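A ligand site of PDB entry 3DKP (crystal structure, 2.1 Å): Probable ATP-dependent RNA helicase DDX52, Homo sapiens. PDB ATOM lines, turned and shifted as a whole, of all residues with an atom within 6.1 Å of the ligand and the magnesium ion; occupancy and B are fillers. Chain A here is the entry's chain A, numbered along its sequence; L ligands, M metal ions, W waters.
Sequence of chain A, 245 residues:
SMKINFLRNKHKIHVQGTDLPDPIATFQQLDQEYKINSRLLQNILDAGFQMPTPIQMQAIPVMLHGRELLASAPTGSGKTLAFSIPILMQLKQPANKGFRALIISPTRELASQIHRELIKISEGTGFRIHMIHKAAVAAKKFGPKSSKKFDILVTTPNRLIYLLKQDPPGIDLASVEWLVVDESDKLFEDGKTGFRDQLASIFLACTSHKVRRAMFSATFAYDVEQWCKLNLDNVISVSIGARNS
Merely in contact with the magnesium ion: Asp 182. The nearest printed residue that does not touch the magnesium ion is Thr 80 (4.1 Å).
Water W1 lies within hydrogen-bond range of OG1 of Thr 80 (2.8 Å) and OD2 of Asp 182 (2.9 Å). Water W11 lies within hydrogen-bond range of OD1 of Asp 182 (2.6 Å) and OE2 of Glu 183 (2.7 Å). Water W7 lies within hydrogen-bond range of O4 of the ligand, N of Leu 81 and OE2 of Glu 117. Water W8 lies within hydrogen-bond range of a nitrogen (N4) of the ligand, the backbone NH of Met 51 and the backbone NH of Gln 50.
N of Lys 79 lies within hydrogen-bond range of O2 of the ligand (3.1 Å). NZ of Lys 79 lies within salt-bridge range of O2 of the ligand (2.5 Å). An oxygen (O3) of the ligand lies within hydrogen-bond range of the backbone NH of Gly 76. NE2 of Gln 56 is in hydrogen-bond range of N2 of the ligand (2.9 Å). O4 of the ligand sits at hydrogen-bond distance from N of Thr 80, 3.0 Å away. OG1 of Thr 80 lies within hydrogen-bond range of O4 of the ligand (2.9 Å). N3 of the ligand is in hydrogen-bond range of O of Met 51 (2.9 Å). The backbone NH (N) of Gly 78 is in hydrogen-bond range of an oxygen (O6) of the ligand (3.0 Å). An oxygen (O2) of the ligand lies within hydrogen-bond range of the backbone NH (N) of Ser 77 (3.1 Å).
The backbone carbonyl oxygen (O) of Pro 74 lies within hydrogen-bond range of the side-chain amino group (NZ) of Lys 79 (3.0 Å). The side-chain amino group of Lys 79 lies within hydrogen-bond range of the backbone carbonyl oxygen of Ala 73 (2.9 Å). NE2 of Gln 56 lies within hydrogen-bond range of O of Gly 78 (2.9 Å). The side-chain amide oxygen (OE1) of Gln 56 lies within hydrogen-bond range of the backbone NH (N) of Thr 53, 2.9 Å away. The side-chain hydroxyl of Ser 77 sits at hydrogen-bond distance from the backbone carbonyl oxygen of Pro 74 (2.5 Å). OG1 of Thr 53 lies within hydrogen-bond range of O of Ser 77, at 2.8 Å.
Merely in contact with the ligand: Phe 49 (3.3 Å), Pro 52 (3.9 Å), Thr 53 (3.8 Å), Pro 74 (3.6 Å), Thr 75 (3.4 Å) and Leu 81 (3.96 Å). Hydrophobic or aromatic side chains within 4 Å of the ligand: Phe 49 and Leu 81. 13 residues have an atom within 4 Å of the ligand: Phe 49, Met 51, Pro 52, Thr 53, Gln 56, Pro 74, Thr 75, Gly 76, Ser 77, Gly 78, Lys 79, Thr 80 and Leu 81.
The magnesium ion is bound by water W4, water W1, O1 of the ligand, water W3, water W2 and water W11.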
ATOM      1  N   PHE A  27      30.068  19.099  31.109  1.00  0.00           N
ATOM      2  CA  PHE A  27      29.996  17.645  31.367  1.00  0.00           C
ATOM      3  C   PHE A  27      30.853  17.195  32.549  1.00  0.00           C
ATOM      4  O   PHE A  27      30.569  16.164  33.181  1.00  0.00           O
ATOM      5  CB  PHE A  27      30.325  16.793  30.130  1.00  0.00           C
ATOM      6  CG  PHE A  27      29.303  16.912  29.040  1.00  0.00           C
ATOM      7  CD1 PHE A  27      27.979  16.540  29.261  1.00  0.00           C
ATOM      8  CD2 PHE A  27      29.661  17.368  27.786  1.00  0.00           C
ATOM      9  CE1 PHE A  27      27.057  16.648  28.246  1.00  0.00           C
ATOM     10  CE2 PHE A  27      28.727  17.480  26.770  1.00  0.00           C
ATOM     11  CZ  PHE A  27      27.437  17.121  26.992  1.00  0.00           C
ATOM     12  N   GLY A  48      33.658  14.988  20.478  1.00  0.00           N
ATOM     13  CA  GLY A  48      33.817  16.411  20.222  1.00  0.00           C
ATOM     14  C   GLY A  48      32.727  17.208  20.923  1.00  0.00           C
ATOM     15  O   GLY A  48      32.548  18.386  20.671  1.00  0.00           O
ATOM     16  N   PHE A  49      31.978  16.555  21.799  1.00  0.00           N
ATOM     17  CA  PHE A  49      30.948  17.262  22.520  1.00  0.00           C
ATOM     18  C   PHE A  49      31.631  17.887  23.700  1.00  0.00           C
ATOM     19  O   PHE A  49      31.599  17.340  24.800  1.00  0.00           O
ATOM     20  CB  PHE A  49      29.833  16.333  22.967  1.00  0.00           C
ATOM     21  CG  PHE A  49      29.224  15.510  21.841  1.00  0.00           C
ATOM     22  CD1 PHE A  49      29.145  16.010  20.539  1.00  0.00           C
ATOM     23  CD2 PHE A  49      28.750  14.241  22.091  1.00  0.00           C
ATOM     24  CE1 PHE A  49      28.560  15.251  19.522  1.00  0.00           C
ATOM     25  CE2 PHE A  49      28.170  13.474  21.071  1.00  0.00           C
ATOM     26  CZ  PHE A  49      28.067  13.983  19.794  1.00  0.00           C
ATOM     27  N   GLN A  50      32.264  19.031  23.444  1.00  0.00           N
ATOM     28  CA  GLN A  50      33.021  19.740  24.460  1.00  0.00           C
ATOM     29  C   GLN A  50      32.156  20.347  25.588  1.00  0.00           C
ATOM     30  O   GLN A  50      32.576  20.409  26.751  1.00  0.00           O
ATOM     31  CB  GLN A  50      33.849  20.817  23.769  1.00  0.00           C
ATOM     32  CG  GLN A  50      34.063  22.078  24.563  1.00  0.00           C
ATOM     33  N   MET A  51      30.938  20.764  25.243  1.00  0.00           N
ATOM     34  CA  MET A  51      30.057  21.480  26.165  1.00  0.00           C
ATOM     35  C   MET A  51      28.608  21.050  25.948  1.00  0.00           C
ATOM     36  O   MET A  51      28.166  20.949  24.823  1.00  0.00           O
ATOM     37  CB  MET A  51      30.161  22.985  25.884  1.00  0.00           C
ATOM     38  CG  MET A  51      31.511  23.616  26.220  1.00  0.00           C
ATOM     39  SD  MET A  51      31.713  23.801  28.000  1.00  0.00           S
ATOM     40  CE  MET A  51      30.132  24.511  28.410  1.00  0.00           C
ATOM     41  N   PRO A  52      27.843  20.818  27.029  1.00  0.00           N
ATOM     42  CA  PRO A  52      26.461  20.451  26.744  1.00  0.00           C
ATOM     43  C   PRO A  52      25.735  21.577  26.066  1.00  0.00           C
ATOM     44  O   PRO A  52      26.046  22.767  26.304  1.00  0.00           O
ATOM     45  CB  PRO A  52      25.847  20.273  28.137  1.00  0.00           C
ATOM     46  CG  PRO A  52      26.784  20.968  29.056  1.00  0.00           C
ATOM     47  CD  PRO A  52      28.140  20.872  28.468  1.00  0.00           C
ATOM     48  N   THR A  53      24.721  21.207  25.295  1.00  0.00           N
ATOM     49  CA  THR A  53      23.854  22.168  24.645  1.00  0.00           C
ATOM     50  C   THR A  53      22.835  22.659  25.675  1.00  0.00           C
ATOM     51  O   THR A  53      22.699  22.061  26.725  1.00  0.00           O
ATOM     52  CB  THR A  53      23.110  21.541  23.459  1.00  0.00           C
ATOM     53  OG1 THR A  53      22.193  20.540  23.931  1.00  0.00           O
ATOM     54  CG2 THR A  53      24.088  20.941  22.465  1.00  0.00           C
ATOM     55  N   ILE A  55      19.616  22.444  25.947  1.00  0.00           N
ATOM     56  CA  ILE A  55      18.615  21.448  26.374  1.00  0.00           C
ATOM     57  C   ILE A  55      19.260  20.374  27.260  1.00  0.00           C
ATOM     58  O   ILE A  55      18.692  19.977  28.285  1.00  0.00           O
ATOM     59  CB  ILE A  55      17.821  20.839  25.163  1.00  0.00           C
ATOM     60  CG1 ILE A  55      16.557  20.104  25.631  1.00  0.00           C
ATOM     61  CG2 ILE A  55      18.670  19.878  24.357  1.00  0.00           C
ATOM     62  CD1 ILE A  55      15.589  20.943  26.491  1.00  0.00           C
ATOM     63  N   GLN A  56      20.445  19.915  26.881  1.00  0.00           N
ATOM     64  CA  GLN A  56      21.252  19.035  27.719  1.00  0.00           C
ATOM     65  C   GLN A  56      21.521  19.646  29.096  1.00  0.00           C
ATOM     66  O   GLN A  56      21.380  18.984  30.108  1.00  0.00           O
ATOM     67  CB  GLN A  56      22.557  18.690  27.017  1.00  0.00           C
ATOM     68  CG  GLN A  56      22.297  17.884  25.723  1.00  0.00           C
ATOM     69  CD  GLN A  56      23.488  17.855  24.787  1.00  0.00           C
ATOM     70  OE1 GLN A  56      24.575  18.352  25.128  1.00  0.00           O
ATOM     71  NE2 GLN A  56      23.270  17.298  23.571  1.00  0.00           N
ATOM     72  N   ALA A  73      12.892  21.808  22.194  1.00  0.00           N
ATOM     73  CA  ALA A  73      13.982  22.558  21.595  1.00  0.00           C
ATOM     74  C   ALA A  73      13.978  22.248  20.093  1.00  0.00           C
ATOM     75  O   ALA A  73      13.699  21.140  19.710  1.00  0.00           O
ATOM     76  CB  ALA A  73      15.310  22.145  22.237  1.00  0.00           C
ATOM     77  N   PRO A  74      14.317  23.238  19.250  1.00  0.00           N
ATOM     78  CA  PRO A  74      14.279  23.032  17.788  1.00  0.00           C
ATOM     79  C   PRO A  74      15.134  21.829  17.353  1.00  0.00           C
ATOM     80  O   PRO A  74      16.009  21.392  18.113  1.00  0.00           O
ATOM     81  CB  PRO A  74      14.876  24.319  17.195  1.00  0.00           C
ATOM     82  CG  PRO A  74      14.822  25.344  18.303  1.00  0.00           C
ATOM     83  CD  PRO A  74      14.756  24.591  19.635  1.00  0.00           C
ATOM     84  N   THR A  75      14.857  21.279  16.188  1.00  0.00           N
ATOM     85  CA  THR A  75      15.791  20.373  15.518  1.00  0.00           C
ATOM     86  C   THR A  75      17.233  20.888  15.557  1.00  0.00           C
ATOM     87  O   THR A  75      17.502  22.076  15.323  1.00  0.00           O
ATOM     88  CB  THR A  75      15.335  20.153  14.034  1.00  0.00           C
ATOM     89  OG1 THR A  75      13.981  19.675  14.022  1.00  0.00           O
ATOM     90  CG2 THR A  75      16.220  19.159  13.307  1.00  0.00           C
ATOM     91  N   GLY A  76      18.189  19.999  15.824  1.00  0.00           N
ATOM     92  CA  GLY A  76      19.587  20.397  15.841  1.00  0.00           C
ATOM     93  C   GLY A  76      20.040  20.804  17.237  1.00  0.00           C
ATOM     94  O   GLY A  76      21.134  21.311  17.408  1.00  0.00           O
ATOM     95  N   SER A  77      19.208  20.588  18.250  1.00  0.00           N
ATOM     96  CA  SER A  77      19.534  21.088  19.562  1.00  0.00           C
ATOM     97  C   SER A  77      20.338  20.121  20.447  1.00  0.00           C
ATOM     98  O   SER A  77      20.791  20.531  21.509  1.00  0.00           O
ATOM     99  CB  SER A  77      18.264  21.493  20.299  1.00  0.00           C
ATOM    100  OG  SER A  77      17.640  22.568  19.626  1.00  0.00           O
ATOM    101  N   GLY A  78      20.470  18.860  20.004  1.00  0.00           N
ATOM    102  CA  GLY A  78      21.085  17.764  20.773  1.00  0.00           C
ATOM    103  C   GLY A  78      20.124  17.053  21.731  1.00  0.00           C
ATOM    104  O   GLY A  78      20.502  16.645  22.837  1.00  0.00           O
ATOM    105  N   LYS A  79      18.865  16.906  21.326  1.00  0.00           N
ATOM    106  CA  LYS A  79      17.896  16.261  22.208  1.00  0.00           C
ATOM    107  C   LYS A  79      18.194  14.764  22.403  1.00  0.00           C
ATOM    108  O   LYS A  79      17.887  14.225  23.463  1.00  0.00           O
ATOM    109  CB  LYS A  79      16.440  16.473  21.719  1.00  0.00           C
ATOM    110  CG  LYS A  79      15.990  17.918  21.770  1.00  0.00           C
ATOM    111  CD  LYS A  79      14.503  18.071  21.479  1.00  0.00           C
ATOM    112  CE  LYS A  79      14.230  17.844  19.985  1.00  0.00           C
ATOM    113  NZ  LYS A  79      15.067  18.718  19.062  1.00  0.00           N
ATOM    114  N   THR A  80      18.836  14.104  21.432  1.00  0.00           N
ATOM    115  CA  THR A  80      19.179  12.687  21.643  1.00  0.00           C
ATOM    116  C   THR A  80      20.089  12.472  22.848  1.00  0.00           C
ATOM    117  O   THR A  80      19.820  11.635  23.686  1.00  0.00           O
ATOM    118  CB  THR A  80      19.808  12.024  20.401  1.00  0.00           C
ATOM    119  OG1 THR A  80      18.966  12.269  19.280  1.00  0.00           O
ATOM    120  CG2 THR A  80      19.929  10.501  20.577  1.00  0.00           C
ATOM    121  N   LEU A  81      21.166  13.254  22.953  1.00  0.00           N
ATOM    122  CA  LEU A  81      22.090  13.042  24.077  1.00  0.00           C
ATOM    123  C   LEU A  81      21.494  13.490  25.394  1.00  0.00           C
ATOM    124  O   LEU A  81      21.828  12.942  26.471  1.00  0.00           O
ATOM    125  CB  LEU A  81      23.361  13.831  23.806  1.00  0.00           C
ATOM    126  CG  LEU A  81      24.618  13.083  24.081  1.00  0.00           C
ATOM    127  CD1 LEU A  81      24.598  11.983  23.053  1.00  0.00           C
ATOM    128  CD2 LEU A  81      25.813  14.089  23.911  1.00  0.00           C
ATOM    129  N   ILE A 114      18.675   7.303  16.536  1.00  0.00           N
ATOM    130  CA  ILE A 114      18.844   7.257  17.985  1.00  0.00           C
ATOM    131  C   ILE A 114      19.655   6.025  18.388  1.00  0.00           C
ATOM    132  O   ILE A 114      20.542   6.087  19.233  1.00  0.00           O
ATOM    133  CB  ILE A 114      17.483   7.246  18.722  1.00  0.00           C
ATOM    134  CG1 ILE A 114      16.780   8.610  18.561  1.00  0.00           C
ATOM    135  CG2 ILE A 114      17.665   6.870  20.180  1.00  0.00           C
ATOM    136  CD1 ILE A 114      15.241   8.550  18.732  1.00  0.00           C
ATOM    137  N   GLU A 117      23.434   6.582  17.739  1.00  0.00           N
ATOM    138  CA  GLU A 117      23.998   7.542  18.670  1.00  0.00           C
ATOM    139  C   GLU A 117      24.243   6.849  20.041  1.00  0.00           C
ATOM    140  O   GLU A 117      25.294   7.016  20.640  1.00  0.00           O
ATOM    141  CB  GLU A 117      23.057   8.735  18.846  1.00  0.00           C
ATOM    142  CG  GLU A 117      23.567   9.790  19.828  1.00  0.00           C
ATOM    143  CD  GLU A 117      24.233  10.971  19.105  1.00  0.00           C
ATOM    144  OE1 GLU A 117      25.143  10.707  18.277  1.00  0.00           O
ATOM    145  OE2 GLU A 117      23.848  12.139  19.356  1.00  0.00           O
ATOM    146  N   LYS A 120      27.170   4.474  19.789  1.00  0.00           N
ATOM    147  CA  LYS A 120      28.450   5.173  19.709  1.00  0.00           C
ATOM    148  C   LYS A 120      28.869   5.752  21.076  1.00  0.00           C
ATOM    149  O   LYS A 120      30.003   5.540  21.505  1.00  0.00           O
ATOM    150  CB  LYS A 120      28.416   6.248  18.617  1.00  0.00           C
ATOM    151  CG  LYS A 120      29.782   6.651  18.068  1.00  0.00           C
ATOM    152  CD  LYS A 120      29.685   8.040  17.446  1.00  0.00           C
ATOM    153  CE  LYS A 120      29.505   9.123  18.527  1.00  0.00           C
ATOM    154  NZ  LYS A 120      28.652  10.232  18.020  1.00  0.00           N
ATOM    155  N   ASP A 182      10.310  10.643  21.846  1.00  0.00           N
ATOM    156  CA  ASP A 182      11.042  11.597  21.053  1.00  0.00           C
ATOM    157  C   ASP A 182      10.144  12.076  19.909  1.00  0.00           C
ATOM    158  O   ASP A 182       9.371  11.294  19.347  1.00  0.00           O
ATOM    159  CB  ASP A 182      12.305  10.927  20.519  1.00  0.00           C
ATOM    160  CG  ASP A 182      13.298  11.907  19.900  1.00  0.00           C
ATOM    161  OD1 ASP A 182      13.338  13.128  20.231  1.00  0.00           O
ATOM    162  OD2 ASP A 182      14.075  11.422  19.062  1.00  0.00           O
ATOM    163  N   GLU A 183      10.263  13.365  19.569  1.00  0.00           N
ATOM    164  CA  GLU A 183       9.357  14.009  18.604  1.00  0.00           C
ATOM    165  C   GLU A 183       7.874  13.836  18.967  1.00  0.00           C
ATOM    166  O   GLU A 183       7.059  13.437  18.127  1.00  0.00           O
ATOM    167  CB  GLU A 183       9.650  13.525  17.169  1.00  0.00           C
ATOM    168  CG  GLU A 183      11.102  13.736  16.703  1.00  0.00           C
ATOM    169  CD  GLU A 183      11.418  15.198  16.391  1.00  0.00           C
ATOM    170  OE1 GLU A 183      11.018  15.658  15.310  1.00  0.00           O
ATOM    171  OE2 GLU A 183      12.067  15.893  17.224  1.00  0.00           O
HETATM  172  P1  LIG L   1      17.822  17.020  17.818  1.00  0.00           P
HETATM  173  O1  LIG L   1      17.237  15.711  18.180  1.00  0.00           O
HETATM  174  O2  LIG L   1      17.476  18.144  18.877  1.00  0.00           O
HETATM  175  O3  LIG L   1      17.435  17.569  16.343  1.00  0.00           O
HETATM  176  P2  LIG L   1      20.363  15.740  17.681  1.00  0.00           P
HETATM  177  O4  LIG L   1      20.254  14.795  18.839  1.00  0.00           O
HETATM  178  O5  LIG L   1      19.990  15.010  16.323  1.00  0.00           O
HETATM  179  O6  LIG L   1      19.445  17.066  17.804  1.00  0.00           O
HETATM  180  O7  LIG L   1      21.823  16.345  17.591  1.00  0.00           O
HETATM  181  C1  LIG L   1      22.144  17.119  16.410  1.00  0.00           C
HETATM  182  C2  LIG L   1      23.667  17.244  16.204  1.00  0.00           C
HETATM  183  O8  LIG L   1      24.223  17.859  17.380  1.00  0.00           O
HETATM  184  C3  LIG L   1      24.212  15.814  16.131  1.00  0.00           C
HETATM  185  O9  LIG L   1      25.165  15.731  15.051  1.00  0.00           O
HETATM  186  C4  LIG L   1      24.901  15.623  17.482  1.00  0.00           C
HETATM  187  O10 LIG L   1      26.079  14.874  17.280  1.00  0.00           O
HETATM  188  C5  LIG L   1      25.324  17.017  17.824  1.00  0.00           C
HETATM  189  N1  LIG L   1      25.459  17.203  19.305  1.00  0.00           N
HETATM  190  C6  LIG L   1      24.704  16.711  20.296  1.00  0.00           C
HETATM  191  N2  LIG L   1      25.184  17.135  21.464  1.00  0.00           N
HETATM  192  C7  LIG L   1      26.245  17.919  21.191  1.00  0.00           C
HETATM  193  C8  LIG L   1      27.136  18.636  21.968  1.00  0.00           C
HETATM  194  N3  LIG L   1      27.039  18.677  23.325  1.00  0.00           N
HETATM  195  N4  LIG L   1      28.100  19.327  21.330  1.00  0.00           N
HETATM  196  C9  LIG L   1      28.227  19.339  20.015  1.00  0.00           C
HETATM  197  N5  LIG L   1      27.398  18.647  19.253  1.00  0.00           N
HETATM  198  C10 LIG L   1      26.410  17.950  19.825  1.00  0.00           C
HETATM  199 MG    MG M   1      16.104  14.356  17.259  1.00  0.00          MG
HETATM  200  O   HOH W   1      16.369  13.094  18.752  1.00  0.00           O
HETATM  201  O   HOH W   2      15.055  12.715  16.295  1.00  0.00           O
HETATM  202  O   HOH W   3      15.681  15.622  15.650  1.00  0.00           O
HETATM  203  O   HOH W   4      17.619  13.591  16.295  1.00  0.00           O
HETATM  204  O   HOH W   5      28.347  18.856  16.498  1.00  0.00           O
HETATM  205  O   HOH W   6      26.440  22.259  20.102  1.00  0.00           O
HETATM  206  O   HOH W   7      22.306  14.420  20.654  1.00  0.00           O
HETATM  207  O   HOH W   8      30.146  21.140  22.131  1.00  0.00           O
HETATM  208  O   HOH W   9      31.112  21.012  19.827  1.00  0.00           O
HETATM  209  O   HOH W  10      18.847  16.681  14.303  1.00  0.00           O
HETATM  210  O   HOH W  11      14.200  14.712  18.323  1.00  0.00           O
